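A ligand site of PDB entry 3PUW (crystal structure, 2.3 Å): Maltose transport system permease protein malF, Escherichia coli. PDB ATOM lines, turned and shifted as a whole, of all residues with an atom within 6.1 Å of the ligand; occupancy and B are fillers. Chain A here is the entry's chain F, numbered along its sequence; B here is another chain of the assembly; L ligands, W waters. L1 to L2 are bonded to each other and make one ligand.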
ATOM      1  N   THR A 291      28.707 -23.888 -14.486  1.00  0.00           N
ATOM      2  CA  THR A 291      28.248 -22.848 -15.407  1.00  0.00           C
ATOM      3  C   THR A 291      28.442 -23.289 -16.862  1.00  0.00           C
ATOM      4  O   THR A 291      27.502 -23.238 -17.653  1.00  0.00           O
ATOM      5  CB  THR A 291      28.956 -21.500 -15.178  1.00  0.00           C
ATOM      6  OG1 THR A 291      28.731 -21.060 -13.840  1.00  0.00           O
ATOM      7  CG2 THR A 291      28.467 -20.436 -16.163  1.00  0.00           C
ATOM      8  N   VAL A 292      29.651 -23.735 -17.196  1.00  0.00           N
ATOM      9  CA  VAL A 292      29.971 -24.162 -18.555  1.00  0.00           C
ATOM     10  C   VAL A 292      29.092 -25.351 -18.960  1.00  0.00           C
ATOM     11  O   VAL A 292      28.454 -25.316 -20.015  1.00  0.00           O
ATOM     12  CB  VAL A 292      31.481 -24.514 -18.714  1.00  0.00           C
ATOM     13  CG1 VAL A 292      31.773 -25.103 -20.101  1.00  0.00           C
ATOM     14  CG2 VAL A 292      32.338 -23.272 -18.489  1.00  0.00           C
ATOM     15  N   THR A 295      25.267 -24.178 -19.210  1.00  0.00           N
ATOM     16  CA  THR A 295      25.062 -23.274 -20.350  1.00  0.00           C
ATOM     17  C   THR A 295      25.192 -24.000 -21.694  1.00  0.00           C
ATOM     18  O   THR A 295      24.385 -23.787 -22.591  1.00  0.00           O
ATOM     19  CB  THR A 295      25.967 -22.020 -20.314  1.00  0.00           C
ATOM     20  OG1 THR A 295      27.342 -22.417 -20.131  1.00  0.00           O
ATOM     21  CG2 THR A 295      25.561 -21.084 -19.184  1.00  0.00           C
ATOM     22  N   TYR A 325      20.315 -12.009 -23.262  1.00  0.00           N
ATOM     23  CA  TYR A 325      21.626 -11.607 -23.731  1.00  0.00           C
ATOM     24  C   TYR A 325      21.561 -10.283 -24.498  1.00  0.00           C
ATOM     25  O   TYR A 325      22.581  -9.649 -24.718  1.00  0.00           O
ATOM     26  CB  TYR A 325      22.190 -12.714 -24.614  1.00  0.00           C
ATOM     27  CG  TYR A 325      23.679 -12.692 -24.881  1.00  0.00           C
ATOM     28  CD1 TYR A 325      24.596 -12.161 -23.949  1.00  0.00           C
ATOM     29  CD2 TYR A 325      24.186 -13.243 -26.059  1.00  0.00           C
ATOM     30  CE1 TYR A 325      25.956 -12.153 -24.219  1.00  0.00           C
ATOM     31  CE2 TYR A 325      25.537 -13.244 -26.336  1.00  0.00           C
ATOM     32  CZ  TYR A 325      26.420 -12.704 -25.416  1.00  0.00           C
ATOM     33  OH  TYR A 325      27.757 -12.734 -25.712  1.00  0.00           O
ATOM     34  N   SER A 329      23.532  -6.920 -18.935  1.00  0.00           N
ATOM     35  CA  SER A 329      23.383  -7.814 -17.784  1.00  0.00           C
ATOM     36  C   SER A 329      23.262  -7.111 -16.438  1.00  0.00           C
ATOM     37  O   SER A 329      22.640  -7.636 -15.529  1.00  0.00           O
ATOM     38  CB  SER A 329      24.520  -8.835 -17.760  1.00  0.00           C
ATOM     39  OG  SER A 329      25.773  -8.206 -17.602  1.00  0.00           O
ATOM     40  N   ILE A 333      20.993  -8.511 -13.281  1.00  0.00           N
ATOM     41  CA  ILE A 333      21.586  -9.052 -12.060  1.00  0.00           C
ATOM     42  C   ILE A 333      20.958  -8.408 -10.824  1.00  0.00           C
ATOM     43  O   ILE A 333      20.572  -9.104  -9.882  1.00  0.00           O
ATOM     44  CB  ILE A 333      23.127  -8.887 -12.066  1.00  0.00           C
ATOM     45  CG1 ILE A 333      23.749  -9.739 -13.187  1.00  0.00           C
ATOM     46  CG2 ILE A 333      23.735  -9.264 -10.705  1.00  0.00           C
ATOM     47  CD1 ILE A 333      25.151  -9.327 -13.598  1.00  0.00           C
ATOM     48  N   ASN A 376      23.652 -17.194 -13.410  1.00  0.00           N
ATOM     49  CA  ASN A 376      24.733 -17.280 -14.395  1.00  0.00           C
ATOM     50  C   ASN A 376      24.350 -18.098 -15.632  1.00  0.00           C
ATOM     51  O   ASN A 376      24.751 -17.766 -16.754  1.00  0.00           O
ATOM     52  CB  ASN A 376      25.980 -17.872 -13.745  1.00  0.00           C
ATOM     53  CG  ASN A 376      27.261 -17.347 -14.351  1.00  0.00           C
ATOM     54  OD1 ASN A 376      27.273 -16.297 -14.988  1.00  0.00           O
ATOM     55  ND2 ASN A 376      28.349 -18.067 -14.143  1.00  0.00           N
ATOM     56  N   THR A 377      23.586 -19.163 -15.419  1.00  0.00           N
ATOM     57  CA  THR A 377      23.064 -19.991 -16.511  1.00  0.00           C
ATOM     58  C   THR A 377      22.068 -19.195 -17.354  1.00  0.00           C
ATOM     59  O   THR A 377      22.025 -19.328 -18.579  1.00  0.00           O
ATOM     60  CB  THR A 377      22.390 -21.274 -15.965  1.00  0.00           C
ATOM     61  OG1 THR A 377      23.336 -22.006 -15.162  1.00  0.00           O
ATOM     62  CG2 THR A 377      21.913 -22.171 -17.102  1.00  0.00           C
ATOM     63  N   LEU A 379      22.161 -15.942 -17.621  1.00  0.00           N
ATOM     64  CA  LEU A 379      23.026 -14.988 -18.313  1.00  0.00           C
ATOM     65  C   LEU A 379      23.730 -15.610 -19.516  1.00  0.00           C
ATOM     66  O   LEU A 379      23.832 -14.976 -20.577  1.00  0.00           O
ATOM     67  CB  LEU A 379      24.068 -14.417 -17.346  1.00  0.00           C
ATOM     68  CG  LEU A 379      23.628 -13.413 -16.269  1.00  0.00           C
ATOM     69  CD1 LEU A 379      24.748 -13.156 -15.281  1.00  0.00           C
ATOM     70  CD2 LEU A 379      23.147 -12.113 -16.893  1.00  0.00           C
ATOM     71  N   GLY A 380      24.212 -16.846 -19.356  1.00  0.00           N
ATOM     72  CA  GLY A 380      25.170 -17.426 -20.304  1.00  0.00           C
ATOM     73  C   GLY A 380      24.688 -18.428 -21.337  1.00  0.00           C
ATOM     74  O   GLY A 380      25.447 -18.759 -22.260  1.00  0.00           O
ATOM     75  N   TYR A 381      23.455 -18.913 -21.210  1.00  0.00           N
ATOM     76  CA  TYR A 381      22.946 -19.921 -22.158  1.00  0.00           C
ATOM     77  C   TYR A 381      22.803 -19.405 -23.607  1.00  0.00           C
ATOM     78  O   TYR A 381      23.039 -20.181 -24.543  1.00  0.00           O
ATOM     79  CB  TYR A 381      21.667 -20.623 -21.668  1.00  0.00           C
ATOM     80  CG  TYR A 381      20.370 -19.878 -21.926  1.00  0.00           C
ATOM     81  CD1 TYR A 381      19.804 -19.842 -23.203  1.00  0.00           C
ATOM     82  CD2 TYR A 381      19.707 -19.230 -20.880  1.00  0.00           C
ATOM     83  CE1 TYR A 381      18.613 -19.157 -23.438  1.00  0.00           C
ATOM     84  CE2 TYR A 381      18.525 -18.537 -21.107  1.00  0.00           C
ATOM     85  CZ  TYR A 381      17.980 -18.507 -22.389  1.00  0.00           C
ATOM     86  OH  TYR A 381      16.801 -17.824 -22.607  1.00  0.00           O
ATOM     87  N   TYR A 383      24.692 -17.338 -25.258  1.00  0.00           N
ATOM     88  CA  TYR A 383      26.017 -17.411 -25.858  1.00  0.00           C
ATOM     89  C   TYR A 383      26.241 -18.766 -26.523  1.00  0.00           C
ATOM     90  O   TYR A 383      26.570 -18.848 -27.713  1.00  0.00           O
ATOM     91  CB  TYR A 383      27.106 -17.161 -24.808  1.00  0.00           C
ATOM     92  CG  TYR A 383      28.509 -17.252 -25.356  1.00  0.00           C
ATOM     93  CD1 TYR A 383      28.998 -16.300 -26.253  1.00  0.00           C
ATOM     94  CD2 TYR A 383      29.351 -18.304 -24.991  1.00  0.00           C
ATOM     95  CE1 TYR A 383      30.294 -16.389 -26.768  1.00  0.00           C
ATOM     96  CE2 TYR A 383      30.653 -18.394 -25.499  1.00  0.00           C
ATOM     97  CZ  TYR A 383      31.106 -17.430 -26.379  1.00  0.00           C
ATOM     98  OH  TYR A 383      32.395 -17.516 -26.888  1.00  0.00           O
ATOM     99  N   MET A 384      26.030 -19.831 -25.745  1.00  0.00           N
ATOM    100  CA  MET A 384      26.188 -21.203 -26.221  1.00  0.00           C
ATOM    101  C   MET A 384      25.129 -21.575 -27.248  1.00  0.00           C
ATOM    102  O   MET A 384      25.422 -22.286 -28.207  1.00  0.00           O
ATOM    103  CB  MET A 384      26.175 -22.189 -25.063  1.00  0.00           C
ATOM    104  CG  MET A 384      27.370 -22.064 -24.139  1.00  0.00           C
ATOM    105  SD  MET A 384      28.929 -22.362 -24.993  1.00  0.00           S
ATOM    106  CE  MET A 384      30.056 -21.761 -23.743  1.00  0.00           C
ATOM    107  N   LEU A 429      35.916 -23.277 -27.063  1.00  0.00           N
ATOM    108  CA  LEU A 429      34.942 -22.310 -26.545  1.00  0.00           C
ATOM    109  C   LEU A 429      34.571 -22.602 -25.096  1.00  0.00           C
ATOM    110  O   LEU A 429      34.333 -21.673 -24.328  1.00  0.00           O
ATOM    111  CB  LEU A 429      33.699 -22.271 -27.420  1.00  0.00           C
ATOM    112  CG  LEU A 429      33.911 -21.677 -28.816  1.00  0.00           C
ATOM    113  CD1 LEU A 429      32.785 -22.064 -29.755  1.00  0.00           C
ATOM    114  CD2 LEU A 429      34.090 -20.157 -28.762  1.00  0.00           C
ATOM    115  N   ALA A 432      37.562 -21.660 -22.878  1.00  0.00           N
ATOM    116  CA  ALA A 432      37.521 -20.205 -22.751  1.00  0.00           C
ATOM    117  C   ALA A 432      36.438 -19.762 -21.763  1.00  0.00           C
ATOM    118  O   ALA A 432      36.693 -18.928 -20.896  1.00  0.00           O
ATOM    119  CB  ALA A 432      37.291 -19.562 -24.101  1.00  0.00           C
ATOM    120  N   SER A 433      35.247 -20.345 -21.899  1.00  0.00           N
ATOM    121  CA  SER A 433      34.135 -20.069 -21.002  1.00  0.00           C
ATOM    122  C   SER A 433      34.464 -20.419 -19.548  1.00  0.00           C
ATOM    123  O   SER A 433      33.961 -19.786 -18.628  1.00  0.00           O
ATOM    124  CB  SER A 433      32.870 -20.781 -21.446  1.00  0.00           C
ATOM    125  OG  SER A 433      31.745 -20.377 -20.686  1.00  0.00           O
ATOM    126  N   PHE A 434      35.317 -21.426 -19.351  1.00  0.00           N
ATOM    127  CA  PHE A 434      35.806 -21.792 -18.023  1.00  0.00           C
ATOM    128  C   PHE A 434      36.667 -20.686 -17.425  1.00  0.00           C
ATOM    129  O   PHE A 434      36.510 -20.343 -16.255  1.00  0.00           O
ATOM    130  CB  PHE A 434      36.591 -23.111 -18.048  1.00  0.00           C
ATOM    131  CG  PHE A 434      37.249 -23.433 -16.731  1.00  0.00           C
ATOM    132  CD1 PHE A 434      38.580 -23.071 -16.493  1.00  0.00           C
ATOM    133  CD2 PHE A 434      36.545 -24.072 -15.724  1.00  0.00           C
ATOM    134  CE1 PHE A 434      39.193 -23.357 -15.276  1.00  0.00           C
ATOM    135  CE2 PHE A 434      37.148 -24.363 -14.486  1.00  0.00           C
ATOM    136  CZ  PHE A 434      38.476 -23.992 -14.271  1.00  0.00           C
ATOM    137  N   PHE A 436      36.816 -17.494 -18.344  1.00  0.00           N
ATOM    138  CA  PHE A 436      36.000 -16.299 -18.173  1.00  0.00           C
ATOM    139  C   PHE A 436      35.226 -16.348 -16.859  1.00  0.00           C
ATOM    140  O   PHE A 436      35.255 -15.393 -16.091  1.00  0.00           O
ATOM    141  CB  PHE A 436      35.033 -16.126 -19.359  1.00  0.00           C
ATOM    142  CG  PHE A 436      34.137 -14.924 -19.238  1.00  0.00           C
ATOM    143  CD1 PHE A 436      32.864 -15.046 -18.669  1.00  0.00           C
ATOM    144  CD2 PHE A 436      34.557 -13.683 -19.680  1.00  0.00           C
ATOM    145  CE1 PHE A 436      32.034 -13.925 -18.547  1.00  0.00           C
ATOM    146  CE2 PHE A 436      33.737 -12.555 -19.566  1.00  0.00           C
ATOM    147  CZ  PHE A 436      32.471 -12.680 -19.003  1.00  0.00           C
ATOM    148  N   ASN A 437      34.542 -17.466 -16.626  1.00  0.00           N
ATOM    149  CA  ASN A 437      33.739 -17.610 -15.418  1.00  0.00           C
ATOM    150  C   ASN A 437      34.571 -17.757 -14.147  1.00  0.00           C
ATOM    151  O   ASN A 437      34.135 -17.340 -13.069  1.00  0.00           O
ATOM    152  CB  ASN A 437      32.743 -18.763 -15.559  1.00  0.00           C
ATOM    153  CG  ASN A 437      31.520 -18.357 -16.359  1.00  0.00           C
ATOM    154  OD1 ASN A 437      31.237 -18.928 -17.421  1.00  0.00           O
ATOM    155  ND2 ASN A 437      30.788 -17.359 -15.872  1.00  0.00           N
ATOM    156  N   ASN A 440      34.815 -14.244 -13.051  1.00  0.00           N
ATOM    157  CA  ASN A 440      33.556 -13.494 -13.120  1.00  0.00           C
ATOM    158  C   ASN A 440      33.318 -12.639 -11.865  1.00  0.00           C
ATOM    159  O   ASN A 440      32.367 -12.851 -11.114  1.00  0.00           O
ATOM    160  CB  ASN A 440      32.395 -14.461 -13.362  1.00  0.00           C
ATOM    161  CG  ASN A 440      31.272 -13.847 -14.196  1.00  0.00           C
ATOM    162  OD1 ASN A 440      30.597 -14.550 -14.958  1.00  0.00           O
ATOM    163  ND2 ASN A 440      31.062 -12.540 -14.060  1.00  0.00           N
ATOM    164  N   LEU A 443      29.606 -10.487 -11.385  1.00  0.00           N
ATOM    165  CA  LEU A 443      28.405 -11.228 -10.962  1.00  0.00           C
ATOM    166  C   LEU A 443      28.326 -11.401  -9.443  1.00  0.00           C
ATOM    167  O   LEU A 443      27.315 -11.075  -8.835  1.00  0.00           O
ATOM    168  CB  LEU A 443      28.330 -12.583 -11.661  1.00  0.00           C
ATOM    169  CG  LEU A 443      27.181 -13.507 -11.241  1.00  0.00           C
ATOM    170  CD1 LEU A 443      25.794 -12.917 -11.540  1.00  0.00           C
ATOM    171  CD2 LEU A 443      27.334 -14.853 -11.914  1.00  0.00           C
ATOM    172  N   LEU B 172      38.999 -15.977 -30.080  1.00  0.00           N
ATOM    173  CA  LEU B 172      37.953 -16.991 -29.984  1.00  0.00           C
ATOM    174  C   LEU B 172      37.210 -17.156 -31.304  1.00  0.00           C
ATOM    175  O   LEU B 172      36.955 -18.280 -31.753  1.00  0.00           O
ATOM    176  CB  LEU B 172      36.979 -16.651 -28.853  1.00  0.00           C
ATOM    177  CG  LEU B 172      37.388 -17.166 -27.458  1.00  0.00           C
ATOM    178  CD1 LEU B 172      36.497 -16.585 -26.397  1.00  0.00           C
ATOM    179  CD2 LEU B 172      37.340 -18.687 -27.437  1.00  0.00           C
ATOM    180  N   LEU B 221      27.448 -12.312 -32.309  1.00  0.00           N
ATOM    181  CA  LEU B 221      28.168 -12.279 -31.040  1.00  0.00           C
ATOM    182  C   LEU B 221      28.971 -11.003 -30.845  1.00  0.00           C
ATOM    183  O   LEU B 221      29.018 -10.464 -29.743  1.00  0.00           O
ATOM    184  CB  LEU B 221      29.060 -13.511 -30.894  1.00  0.00           C
ATOM    185  CG  LEU B 221      28.368 -14.849 -30.572  1.00  0.00           C
ATOM    186  CD1 LEU B 221      29.375 -15.982 -30.590  1.00  0.00           C
ATOM    187  CD2 LEU B 221      27.647 -14.828 -29.226  1.00  0.00           C
ATOM    188  N   ALA B 225      28.345  -7.904 -28.131  1.00  0.00           N
ATOM    189  CA  ALA B 225      29.494  -7.472 -27.332  1.00  0.00           C
ATOM    190  C   ALA B 225      29.670  -5.961 -27.391  1.00  0.00           C
ATOM    191  O   ALA B 225      29.788  -5.301 -26.353  1.00  0.00           O
ATOM    192  CB  ALA B 225      30.751  -8.172 -27.790  1.00  0.00           C
HETATM  193  C1  LIG L   1      32.440 -14.249 -24.189  1.00  0.00           C
HETATM  194  C2  LIG L   1      31.110 -13.559 -24.480  1.00  0.00           C
HETATM  195  C3  LIG L   1      30.315 -13.322 -23.185  1.00  0.00           C
HETATM  196  C4  LIG L   1      30.135 -14.614 -22.401  1.00  0.00           C
HETATM  197  C5  LIG L   1      31.474 -15.346 -22.212  1.00  0.00           C
HETATM  198  C6  LIG L   1      31.208 -16.752 -21.709  1.00  0.00           C
HETATM  199  O1  LIG L   1      33.331 -13.384 -23.483  1.00  0.00           O
HETATM  200  O2  LIG L   1      31.330 -12.298 -25.121  1.00  0.00           O
HETATM  201  O3  LIG L   1      29.049 -12.758 -23.506  1.00  0.00           O
HETATM  202  O4  LIG L   1      29.606 -14.329 -21.102  1.00  0.00           O
HETATM  203  O5  LIG L   1      32.239 -15.442 -23.425  1.00  0.00           O
HETATM  204  O6  LIG L   1      32.464 -17.420 -21.549  1.00  0.00           O
HETATM  205  C1  LG2 L   2      28.206 -14.605 -20.942  1.00  0.00           C
HETATM  206  C2  LG2 L   2      27.529 -13.435 -20.204  1.00  0.00           C
HETATM  207  C3  LG2 L   2      28.085 -13.291 -18.791  1.00  0.00           C
HETATM  208  C4  LG2 L   2      27.951 -14.608 -18.021  1.00  0.00           C
HETATM  209  C5  LG2 L   2      28.537 -15.769 -18.839  1.00  0.00           C
HETATM  210  C6  LG2 L   2      28.275 -17.122 -18.191  1.00  0.00           C
HETATM  211  O1  LG2 L   2      27.711 -12.211 -20.924  1.00  0.00           O
HETATM  212  O2  LG2 L   2      27.394 -12.247 -18.113  1.00  0.00           O
HETATM  213  O3  LG2 L   2      28.633 -14.483 -16.773  1.00  0.00           O
HETATM  214  O4  LG2 L   2      28.010 -15.800 -20.169  1.00  0.00           O
HETATM  215  O5  LG2 L   2      29.230 -18.071 -18.692  1.00  0.00           O
HETATM  216  O   HOH W   1      28.901 -11.966 -15.507  1.00  0.00           O
HETATM  217  O   HOH W   2      29.068  -9.436 -24.573  1.00  0.00           O
HETATM  218  O   HOH W   3      29.338 -11.679 -27.422  1.00  0.00           O
HETATM  219  O   HOH W   4      33.539 -18.762 -24.424  1.00  0.00           O
HETATM  220  O   HOH W   5      31.610 -12.980 -28.020  1.00  0.00           O
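OD1 of Asn 440 is in hydrogen-bond range of ND2 of Asn 437 (3.0 Å). The side-chain amide nitrogen (ND2) of Asn 437 lies close to the side-chain amide nitrogen (ND2) of Asn 376, 3.1 Å away. The side-chain amide oxygen (OD1) of Asn 437 lies close to the backbone carbonyl oxygen (O) of Ser 433 (3.1 Å). The side-chain amide nitrogen of Asn 376 is in hydrogen-bond range of the side-chain hydroxyl of Thr 291, at 3.0 Å. The side-chain hydroxyl of Thr 295 is in hydrogen-bond range of the backbone carbonyl oxygen of Thr 291, at 2.6 Å.
The side-chain amide oxygen (OD1) of Asn 437 sits at hydrogen-bond distance from an oxygen (O5) of LG2 L2. The side-chain hydroxyl of Tyr 325 is in hydrogen-bond range of an oxygen (O3) of LIG L1, at 2.6 Å. The side-chain amide oxygen (OD1) of Asn 440 lies within hydrogen-bond range of an oxygen (O3) of LG2 L2. The side-chain amide oxygen (OD1) of Asn 376 lies within hydrogen-bond range of an oxygen (O3) of LG2 L2 (2.9 Å). The side-chain hydroxyl (OG) of Ser 433 lies within hydrogen-bond range of an oxygen (O6) of LIG L1, 3.2 Å away.
Water W1 bridges the side-chain amide nitrogen of Asn 440 and an oxygen (O3) of LG2 L2. Water W3 lies within hydrogen-bond range of the side-chain hydroxyl of Tyr 325 (2.6 Å), the backbone carbonyl oxygen of Leu 221 of chain B (2.6 Å) and an oxygen (O2) of LIG L1 (3.1 Å). Water W4 lies within hydrogen-bond range of the side-chain hydroxyl of Tyr 383 (3.0 Å), the backbone carbonyl oxygen of Leu 429 (3.0 Å), an oxygen (O6) of LIG L1 (3.3 Å) and the backbone NH of Ser 433 (3.4 Å).
CG2 of Thr 291 touches O5 of LG2 L2, 3.5 Å away. CB of Leu 379 touches C4 of LG2 L2, 3.9 Å away. Gly 380 touches the ligand. Tyr 383 touches the ligand. CE1 of Phe 436 touches O4 of LIG L1 (3.5 Å). Hydrophobic or aromatic side chains that line the ligand: Tyr 325, Leu 379, Tyr 383 and Phe 436. Within 4 Å of the ligand: Thr 291, Tyr 325, Asn 376, Leu 379, Gly 380, Tyr 383, Ser 433, Phe 436, Asn 437 and Asn 440. The nearest printed residue that does not touch the ligand is Ser 329 (4.4 Å).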
